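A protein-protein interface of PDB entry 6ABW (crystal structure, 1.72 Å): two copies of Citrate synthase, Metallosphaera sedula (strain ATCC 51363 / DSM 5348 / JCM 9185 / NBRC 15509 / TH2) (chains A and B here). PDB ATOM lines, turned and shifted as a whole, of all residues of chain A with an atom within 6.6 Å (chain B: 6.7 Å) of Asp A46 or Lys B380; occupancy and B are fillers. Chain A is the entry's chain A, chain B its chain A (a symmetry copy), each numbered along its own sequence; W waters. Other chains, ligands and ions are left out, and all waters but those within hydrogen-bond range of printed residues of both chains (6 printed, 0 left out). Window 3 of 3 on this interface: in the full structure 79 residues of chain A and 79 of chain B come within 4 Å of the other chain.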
ATOM      1  N   ILE A  39      32.080 -20.324 -13.117  1.00  0.00           N
ATOM      2  CA  ILE A  39      31.098 -19.245 -13.045  1.00  0.00           C
ATOM      3  C   ILE A  39      31.589 -18.069 -13.849  1.00  0.00           C
ATOM      4  O   ILE A  39      32.737 -17.688 -13.732  1.00  0.00           O
ATOM      5  CB  ILE A  39      30.856 -18.770 -11.605  1.00  0.00           C
ATOM      6  CG1 ILE A  39      30.359 -19.950 -10.725  1.00  0.00           C
ATOM      7  CG2 ILE A  39      29.898 -17.562 -11.566  1.00  0.00           C
ATOM      8  CD1 ILE A  39      30.297 -19.586  -9.262  1.00  0.00           C
ATOM      9  N   LEU A  40      30.691 -17.548 -14.683  1.00  0.00           N
ATOM     10  CA  LEU A  40      30.948 -16.362 -15.475  1.00  0.00           C
ATOM     11  C   LEU A  40      29.723 -15.440 -15.291  1.00  0.00           C
ATOM     12  O   LEU A  40      28.570 -15.859 -15.532  1.00  0.00           O
ATOM     13  CB  LEU A  40      31.102 -16.752 -16.961  1.00  0.00           C
ATOM     14  CG  LEU A  40      31.248 -15.532 -17.827  1.00  0.00           C
ATOM     15  CD1 LEU A  40      32.415 -14.657 -17.529  1.00  0.00           C
ATOM     16  CD2 LEU A  40      31.246 -15.990 -19.290  1.00  0.00           C
ATOM     17  N   ARG A  41      29.980 -14.223 -14.844  1.00  0.00           N
ATOM     18  CA  ARG A  41      28.941 -13.190 -14.705  1.00  0.00           C
ATOM     19  C   ARG A  41      29.347 -11.920 -15.390  1.00  0.00           C
ATOM     20  O   ARG A  41      30.489 -11.568 -15.360  1.00  0.00           O
ATOM     21  CB  ARG A  41      28.655 -12.822 -13.248  1.00  0.00           C
ATOM     22  CG  ARG A  41      28.179 -14.030 -12.462  1.00  0.00           C
ATOM     23  CD  ARG A  41      27.942 -13.643 -11.041  1.00  0.00           C
ATOM     24  NE  ARG A  41      27.764 -14.862 -10.281  1.00  0.00           N
ATOM     25  CZ  ARG A  41      28.260 -15.069  -9.070  1.00  0.00           C
ATOM     26  NH1 ARG A  41      28.008 -16.253  -8.501  1.00  0.00           N
ATOM     27  NH2 ARG A  41      28.924 -14.118  -8.404  1.00  0.00           N
ATOM     28  N   TYR A  42      28.382 -11.249 -15.999  1.00  0.00           N
ATOM     29  CA  TYR A  42      28.546  -9.883 -16.497  1.00  0.00           C
ATOM     30  C   TYR A  42      27.725  -8.983 -15.522  1.00  0.00           C
ATOM     31  O   TYR A  42      26.512  -9.137 -15.451  1.00  0.00           O
ATOM     32  CB  TYR A  42      27.988  -9.699 -17.877  1.00  0.00           C
ATOM     33  CG  TYR A  42      28.695 -10.440 -19.041  1.00  0.00           C
ATOM     34  CD1 TYR A  42      30.015 -10.886 -18.944  1.00  0.00           C
ATOM     35  CD2 TYR A  42      27.991 -10.747 -20.163  1.00  0.00           C
ATOM     36  CE1 TYR A  42      30.636 -11.577 -20.002  1.00  0.00           C
ATOM     37  CE2 TYR A  42      28.570 -11.436 -21.236  1.00  0.00           C
ATOM     38  CZ  TYR A  42      29.888 -11.865 -21.163  1.00  0.00           C
ATOM     39  OH  TYR A  42      30.465 -12.504 -22.260  1.00  0.00           O
ATOM     40  N   GLY A  44      27.282  -8.912 -12.482  1.00  0.00           N
ATOM     41  CA  GLY A  44      26.604  -9.720 -11.438  1.00  0.00           C
ATOM     42  C   GLY A  44      25.590 -10.725 -11.927  1.00  0.00           C
ATOM     43  O   GLY A  44      25.092 -11.565 -11.127  1.00  0.00           O
ATOM     44  N   TYR A  45      25.284 -10.706 -13.235  1.00  0.00           N
ATOM     45  CA  TYR A  45      24.325 -11.569 -13.794  1.00  0.00           C
ATOM     46  C   TYR A  45      25.016 -12.800 -14.439  1.00  0.00           C
ATOM     47  O   TYR A  45      25.941 -12.644 -15.248  1.00  0.00           O
ATOM     48  CB  TYR A  45      23.495 -10.850 -14.857  1.00  0.00           C
ATOM     49  CG  TYR A  45      22.679  -9.722 -14.333  1.00  0.00           C
ATOM     50  CD1 TYR A  45      21.552  -9.991 -13.535  1.00  0.00           C
ATOM     51  CD2 TYR A  45      22.977  -8.401 -14.627  1.00  0.00           C
ATOM     52  CE1 TYR A  45      20.741  -8.988 -13.092  1.00  0.00           C
ATOM     53  CE2 TYR A  45      22.148  -7.367 -14.195  1.00  0.00           C
ATOM     54  CZ  TYR A  45      21.043  -7.686 -13.385  1.00  0.00           C
ATOM     55  OH  TYR A  45      20.197  -6.695 -12.931  1.00  0.00           O
ATOM     56  N   ASP A  46      24.599 -14.004 -14.045  1.00  0.00           N
ATOM     57  CA  ASP A  46      25.186 -15.240 -14.560  1.00  0.00           C
ATOM     58  C   ASP A  46      24.989 -15.295 -16.059  1.00  0.00           C
ATOM     59  O   ASP A  46      23.921 -14.979 -16.572  1.00  0.00           O
ATOM     60  CB  ASP A  46      24.518 -16.450 -13.909  1.00  0.00           C
ATOM     61  CG  ASP A  46      25.092 -16.791 -12.537  1.00  0.00           C
ATOM     62  OD1 ASP A  46      26.328 -17.024 -12.386  1.00  0.00           O
ATOM     63  OD2 ASP A  46      24.299 -16.883 -11.575  1.00  0.00           O
ATOM     64  N   ILE A  47      26.000 -15.770 -16.759  1.00  0.00           N
ATOM     65  CA  ILE A  47      25.910 -15.811 -18.238  1.00  0.00           C
ATOM     66  C   ILE A  47      24.738 -16.628 -18.728  1.00  0.00           C
ATOM     67  O   ILE A  47      24.102 -16.231 -19.700  1.00  0.00           O
ATOM     68  CB  ILE A  47      27.254 -16.309 -18.875  1.00  0.00           C
ATOM     69  CG1 ILE A  47      27.217 -16.222 -20.374  1.00  0.00           C
ATOM     70  CG2 ILE A  47      27.619 -17.709 -18.476  1.00  0.00           C
ATOM     71  CD1 ILE A  47      27.352 -14.812 -20.916  1.00  0.00           C
ATOM     72  N   GLU A  48      24.417 -17.744 -18.083  1.00  0.00           N
ATOM     73  CA  GLU A  48      23.275 -18.586 -18.490  1.00  0.00           C
ATOM     74  C   GLU A  48      21.939 -17.811 -18.455  1.00  0.00           C
ATOM     75  O   GLU A  48      21.093 -17.946 -19.361  1.00  0.00           O
ATOM     76  CB  GLU A  48      23.261 -19.883 -17.626  1.00  0.00           C
ATOM     77  CG  GLU A  48      22.263 -20.878 -18.220  1.00  0.00           C
ATOM     78  CD  GLU A  48      22.042 -22.144 -17.393  1.00  0.00           C
ATOM     79  OE1 GLU A  48      22.904 -22.453 -16.535  1.00  0.00           O
ATOM     80  OE2 GLU A  48      20.978 -22.807 -17.616  1.00  0.00           O
ATOM     81  N   ASP A  49      21.770 -17.000 -17.408  1.00  0.00           N
ATOM     82  CA  ASP A  49      20.569 -16.171 -17.112  1.00  0.00           C
ATOM     83  C   ASP A  49      20.484 -15.101 -18.197  1.00  0.00           C
ATOM     84  O   ASP A  49      19.378 -14.832 -18.764  1.00  0.00           O
ATOM     85  CB  ASP A  49      20.768 -15.585 -15.688  1.00  0.00           C
ATOM     86  CG  ASP A  49      19.441 -15.055 -14.978  1.00  0.00           C
ATOM     87  OD1 ASP A  49      18.277 -15.212 -15.523  1.00  0.00           O
ATOM     88  OD2 ASP A  49      19.636 -14.437 -13.883  1.00  0.00           O
ATOM     89  N   LEU A  50      21.629 -14.466 -18.507  1.00  0.00           N
ATOM     90  CA  LEU A  50      21.593 -13.464 -19.574  1.00  0.00           C
ATOM     91  C   LEU A  50      21.209 -14.041 -20.897  1.00  0.00           C
ATOM     92  O   LEU A  50      20.418 -13.433 -21.694  1.00  0.00           O
ATOM     93  CB  LEU A  50      22.942 -12.735 -19.664  1.00  0.00           C
ATOM     94  CG  LEU A  50      23.214 -11.851 -18.462  1.00  0.00           C
ATOM     95  CD1 LEU A  50      24.649 -11.369 -18.568  1.00  0.00           C
ATOM     96  CD2 LEU A  50      22.210 -10.683 -18.363  1.00  0.00           C
ATOM     97  N   VAL A  51      21.759 -15.220 -21.217  1.00  0.00           N
ATOM     98  CA  VAL A  51      21.481 -15.756 -22.577  1.00  0.00           C
ATOM     99  C   VAL A  51      20.022 -16.153 -22.695  1.00  0.00           C
ATOM    100  O   VAL A  51      19.347 -15.835 -23.687  1.00  0.00           O
ATOM    101  CB  VAL A  51      22.402 -16.927 -22.971  1.00  0.00           C
ATOM    102  CG1 VAL A  51      21.882 -17.638 -24.244  1.00  0.00           C
ATOM    103  CG2 VAL A  51      23.800 -16.419 -23.256  1.00  0.00           C
ATOM    104  N   TYR B 375      38.082  -7.797 -10.231  1.00  0.00           N
ATOM    105  CA  TYR B 375      36.646  -7.541 -10.199  1.00  0.00           C
ATOM    106  C   TYR B 375      36.210  -6.741  -8.973  1.00  0.00           C
ATOM    107  O   TYR B 375      36.434  -7.188  -7.879  1.00  0.00           O
ATOM    108  CB  TYR B 375      35.836  -8.827 -10.191  1.00  0.00           C
ATOM    109  CG  TYR B 375      34.376  -8.599 -10.387  1.00  0.00           C
ATOM    110  CD1 TYR B 375      33.882  -8.076 -11.581  1.00  0.00           C
ATOM    111  CD2 TYR B 375      33.456  -8.842  -9.357  1.00  0.00           C
ATOM    112  CE1 TYR B 375      32.542  -7.863 -11.777  1.00  0.00           C
ATOM    113  CE2 TYR B 375      32.098  -8.616  -9.541  1.00  0.00           C
ATOM    114  CZ  TYR B 375      31.630  -8.118 -10.728  1.00  0.00           C
ATOM    115  OH  TYR B 375      30.295  -7.950 -10.899  1.00  0.00           O
ATOM    116  N   PRO B 378      29.294  -5.577  -9.070  1.00  0.00           N
ATOM    117  CA  PRO B 378      28.208  -6.133  -8.292  1.00  0.00           C
ATOM    118  C   PRO B 378      28.315  -7.603  -7.941  1.00  0.00           C
ATOM    119  O   PRO B 378      28.768  -8.439  -8.746  1.00  0.00           O
ATOM    120  CB  PRO B 378      27.002  -5.943  -9.188  1.00  0.00           C
ATOM    121  CG  PRO B 378      27.360  -4.818 -10.076  1.00  0.00           C
ATOM    122  CD  PRO B 378      28.808  -4.918 -10.308  1.00  0.00           C
ATOM    123  N   LEU B 379      27.808  -7.926  -6.749  1.00  0.00           N
ATOM    124  CA  LEU B 379      27.560  -9.287  -6.377  1.00  0.00           C
ATOM    125  C   LEU B 379      26.440  -9.925  -7.213  1.00  0.00           C
ATOM    126  O   LEU B 379      25.681  -9.258  -7.941  1.00  0.00           O
ATOM    127  CB  LEU B 379      27.272  -9.373  -4.852  1.00  0.00           C
ATOM    128  CG  LEU B 379      28.451  -8.875  -4.010  1.00  0.00           C
ATOM    129  CD1 LEU B 379      28.141  -8.941  -2.534  1.00  0.00           C
ATOM    130  CD2 LEU B 379      29.698  -9.684  -4.322  1.00  0.00           C
ATOM    131  N   LYS B 380      26.340 -11.247  -7.087  1.00  0.00           N
ATOM    132  CA  LYS B 380      25.360 -12.058  -7.779  1.00  0.00           C
ATOM    133  C   LYS B 380      23.961 -11.468  -7.725  1.00  0.00           C
ATOM    134  O   LYS B 380      23.504 -11.132  -6.649  1.00  0.00           O
ATOM    135  CB  LYS B 380      25.329 -13.424  -7.101  1.00  0.00           C
ATOM    136  CG  LYS B 380      25.048 -14.576  -7.989  1.00  0.00           C
ATOM    137  CD  LYS B 380      23.649 -14.687  -8.497  1.00  0.00           C
ATOM    138  CE  LYS B 380      23.362 -16.175  -8.713  1.00  0.00           C
ATOM    139  NZ  LYS B 380      22.288 -16.324  -9.723  1.00  0.00           N
ATOM    140  N   ARG B 381      23.273 -11.377  -8.861  1.00  0.00           N
ATOM    141  CA  ARG B 381      21.901 -10.892  -8.896  1.00  0.00           C
ATOM    142  C   ARG B 381      21.199 -11.561 -10.042  1.00  0.00           C
ATOM    143  O   ARG B 381      21.845 -12.101 -10.966  1.00  0.00           O
ATOM    144  CB  ARG B 381      21.853  -9.382  -8.983  1.00  0.00           C
ATOM    145  CG  ARG B 381      22.675  -8.767 -10.125  1.00  0.00           C
ATOM    146  CD  ARG B 381      22.531  -7.243 -10.125  1.00  0.00           C
ATOM    147  NE  ARG B 381      23.441  -6.567 -11.057  1.00  0.00           N
ATOM    148  CZ  ARG B 381      23.350  -5.300 -11.466  1.00  0.00           C
ATOM    149  NH1 ARG B 381      24.222  -4.808 -12.357  1.00  0.00           N
ATOM    150  NH2 ARG B 381      22.360  -4.523 -11.016  1.00  0.00           N
ATOM    151  N   ASP B 382      19.879 -11.594  -9.964  1.00  0.00           N
ATOM    152  CA  ASP B 382      19.078 -12.382 -10.851  1.00  0.00           C
ATOM    153  C   ASP B 382      18.476 -11.436 -11.879  1.00  0.00           C
ATOM    154  O   ASP B 382      18.110 -10.315 -11.530  1.00  0.00           O
ATOM    155  CB  ASP B 382      17.930 -13.103 -10.087  1.00  0.00           C
ATOM    156  CG  ASP B 382      18.426 -14.194  -9.125  1.00  0.00           C
ATOM    157  OD1 ASP B 382      19.589 -14.640  -9.195  1.00  0.00           O
ATOM    158  OD2 ASP B 382      17.602 -14.644  -8.305  1.00  0.00           O
ATOM    159  N   VAL B 383      18.317 -11.910 -13.108  1.00  0.00           N
ATOM    160  CA  VAL B 383      17.720 -11.089 -14.144  1.00  0.00           C
ATOM    161  C   VAL B 383      16.240 -10.943 -13.763  1.00  0.00           C
ATOM    162  O   VAL B 383      15.576 -11.919 -13.422  1.00  0.00           O
ATOM    163  CB  VAL B 383      17.787 -11.695 -15.569  1.00  0.00           C
ATOM    164  CG1 VAL B 383      16.897 -10.935 -16.556  1.00  0.00           C
ATOM    165  CG2 VAL B 383      19.221 -11.742 -16.101  1.00  0.00           C
HETATM  166  O   HOH W   1      22.054 -14.160 -12.772  1.00  0.00           O
HETATM  167  O   HOH W   2      16.215 -14.664 -14.118  1.00  0.00           O
HETATM  168  O   HOH W   3      29.602 -11.208  -8.963  1.00  0.00           O
HETATM  169  O   HOH W   4      30.005  -9.751 -12.868  1.00  0.00           O
HETATM  170  O   HOH W   5      20.453  -4.254 -13.919  1.00  0.00           O
HETATM  171  O   HOH W   6      28.197 -12.782  -5.372  1.00  0.00           O
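Among the printed residues, pairs that only touch across the chains: Arg A41 with Lys B380 (3.4 Å), Gly A44 with Tyr B375 (3.5 Å), Gly A44 with Pro B378 (3.7 Å), Gly A44 with Leu B379 (3.6 Å), Gly A44 with Lys B380 (3.4 Å), Tyr A45 with Arg B381 (3.3 Å), Tyr A45 with Asp B382 (3.3 Å), Tyr A45 with Val B383 (3.8 Å), Asp A49 with Asp B382 (3.7 Å) and Leu A50 with Val B383 (3.9 Å).
Of the printed residues of chain B, Arg A41 touches Lys B380.
Of the printed residues of chain B, Gly A44 touches Tyr B375 (3.5 Å), Pro B378 (3.7 Å), Leu B379 (3.6 Å), Lys B380 (3.4 Å) and Arg B381 (2.9 Å).
Asp A46 touches one residue of chain B.
Printed residues of chain B within 4 Å of Leu A50: Val B383 (3.9 Å).
Printed residues of chain A within 4 Å of Tyr B375: Gly A44.
Of the printed residues of chain A, Pro B378 touches Gly A44 (3.7 Å).
Of the printed residues of chain A, Lys B380 touches Arg A41, Gly A44 and Asp A46.
The nearest residue of chain B that does not touch Asp A46 is Arg B381 (4.5 Å).
The nearest printed residue of chain A that does not touch Pro B378 is Arg A41 (5.7 Å).
NE of Arg A41 is in salt-bridge range of OD1 of Asp A46 (3.3 Å).
The side-chain hydroxyl (OH) of Tyr B375 lies within hydrogen-bond range of the backbone carbonyl oxygen (O) of Pro B378 (2.7 Å).
The side-chain amino group of Lys B380 is in salt-bridge range of the side-chain carboxylate of Asp B382, at 3.2 Å.
Hydrophobic or aromatic side chains of chain B that line the printed part of chain A: Tyr B375 and Val B383.
Along chain B the printed residues that touch a printed residue of chain A span positions 375 to 383.
Among the printed residues, 13 pairs touch across the chains.
The backbone carbonyl oxygen (O) of Gly A44 is in hydrogen-bond range of the backbone NH (N) of Arg B381 (2.9 Å).
The side-chain amino group of Lys B380 lies within salt-bridge range of the side-chain carboxylate of Asp A46 (2.8 Å).
The backbone NH (N) of Val B383 lies within hydrogen-bond range of the side-chain carboxylate (OD2) of Asp A49 (3.0 Å).
No position is printed for both chains.
Water W2 lies within hydrogen-bond range of the side-chain carboxylate of Asp A49 (2.6 Å) and the backbone carbonyl oxygen of Val B383 (2.9 Å).
Water W5 lies within hydrogen-bond range of the side-chain hydroxyl (OH) of Tyr A45 (2.6 Å) and the guanidinium group (NH2) of Arg B381 (3.5 Å).
Water W1 lies within hydrogen-bond range of the side-chain carboxylate (OD2) of Asp A49 (2.7 Å), the backbone carbonyl oxygen (O) of Arg B381 (2.7 Å) and the backbone NH (N) of Asp A46 (2.8 Å).
Water W4 lies within hydrogen-bond range of OH of Tyr B375 (2.7 Å), N of Gly A44 (2.9 Å) and O of Arg A41 (3.1 Å).
Water W3 lies within hydrogen-bond range of O of Pro B378 (2.9 Å) and NH2 of Arg A41 (3.0 Å).
Water W6 bridges N of Lys B380 (3.0 Å) and NH2 of Arg A41 (3.4 Å).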
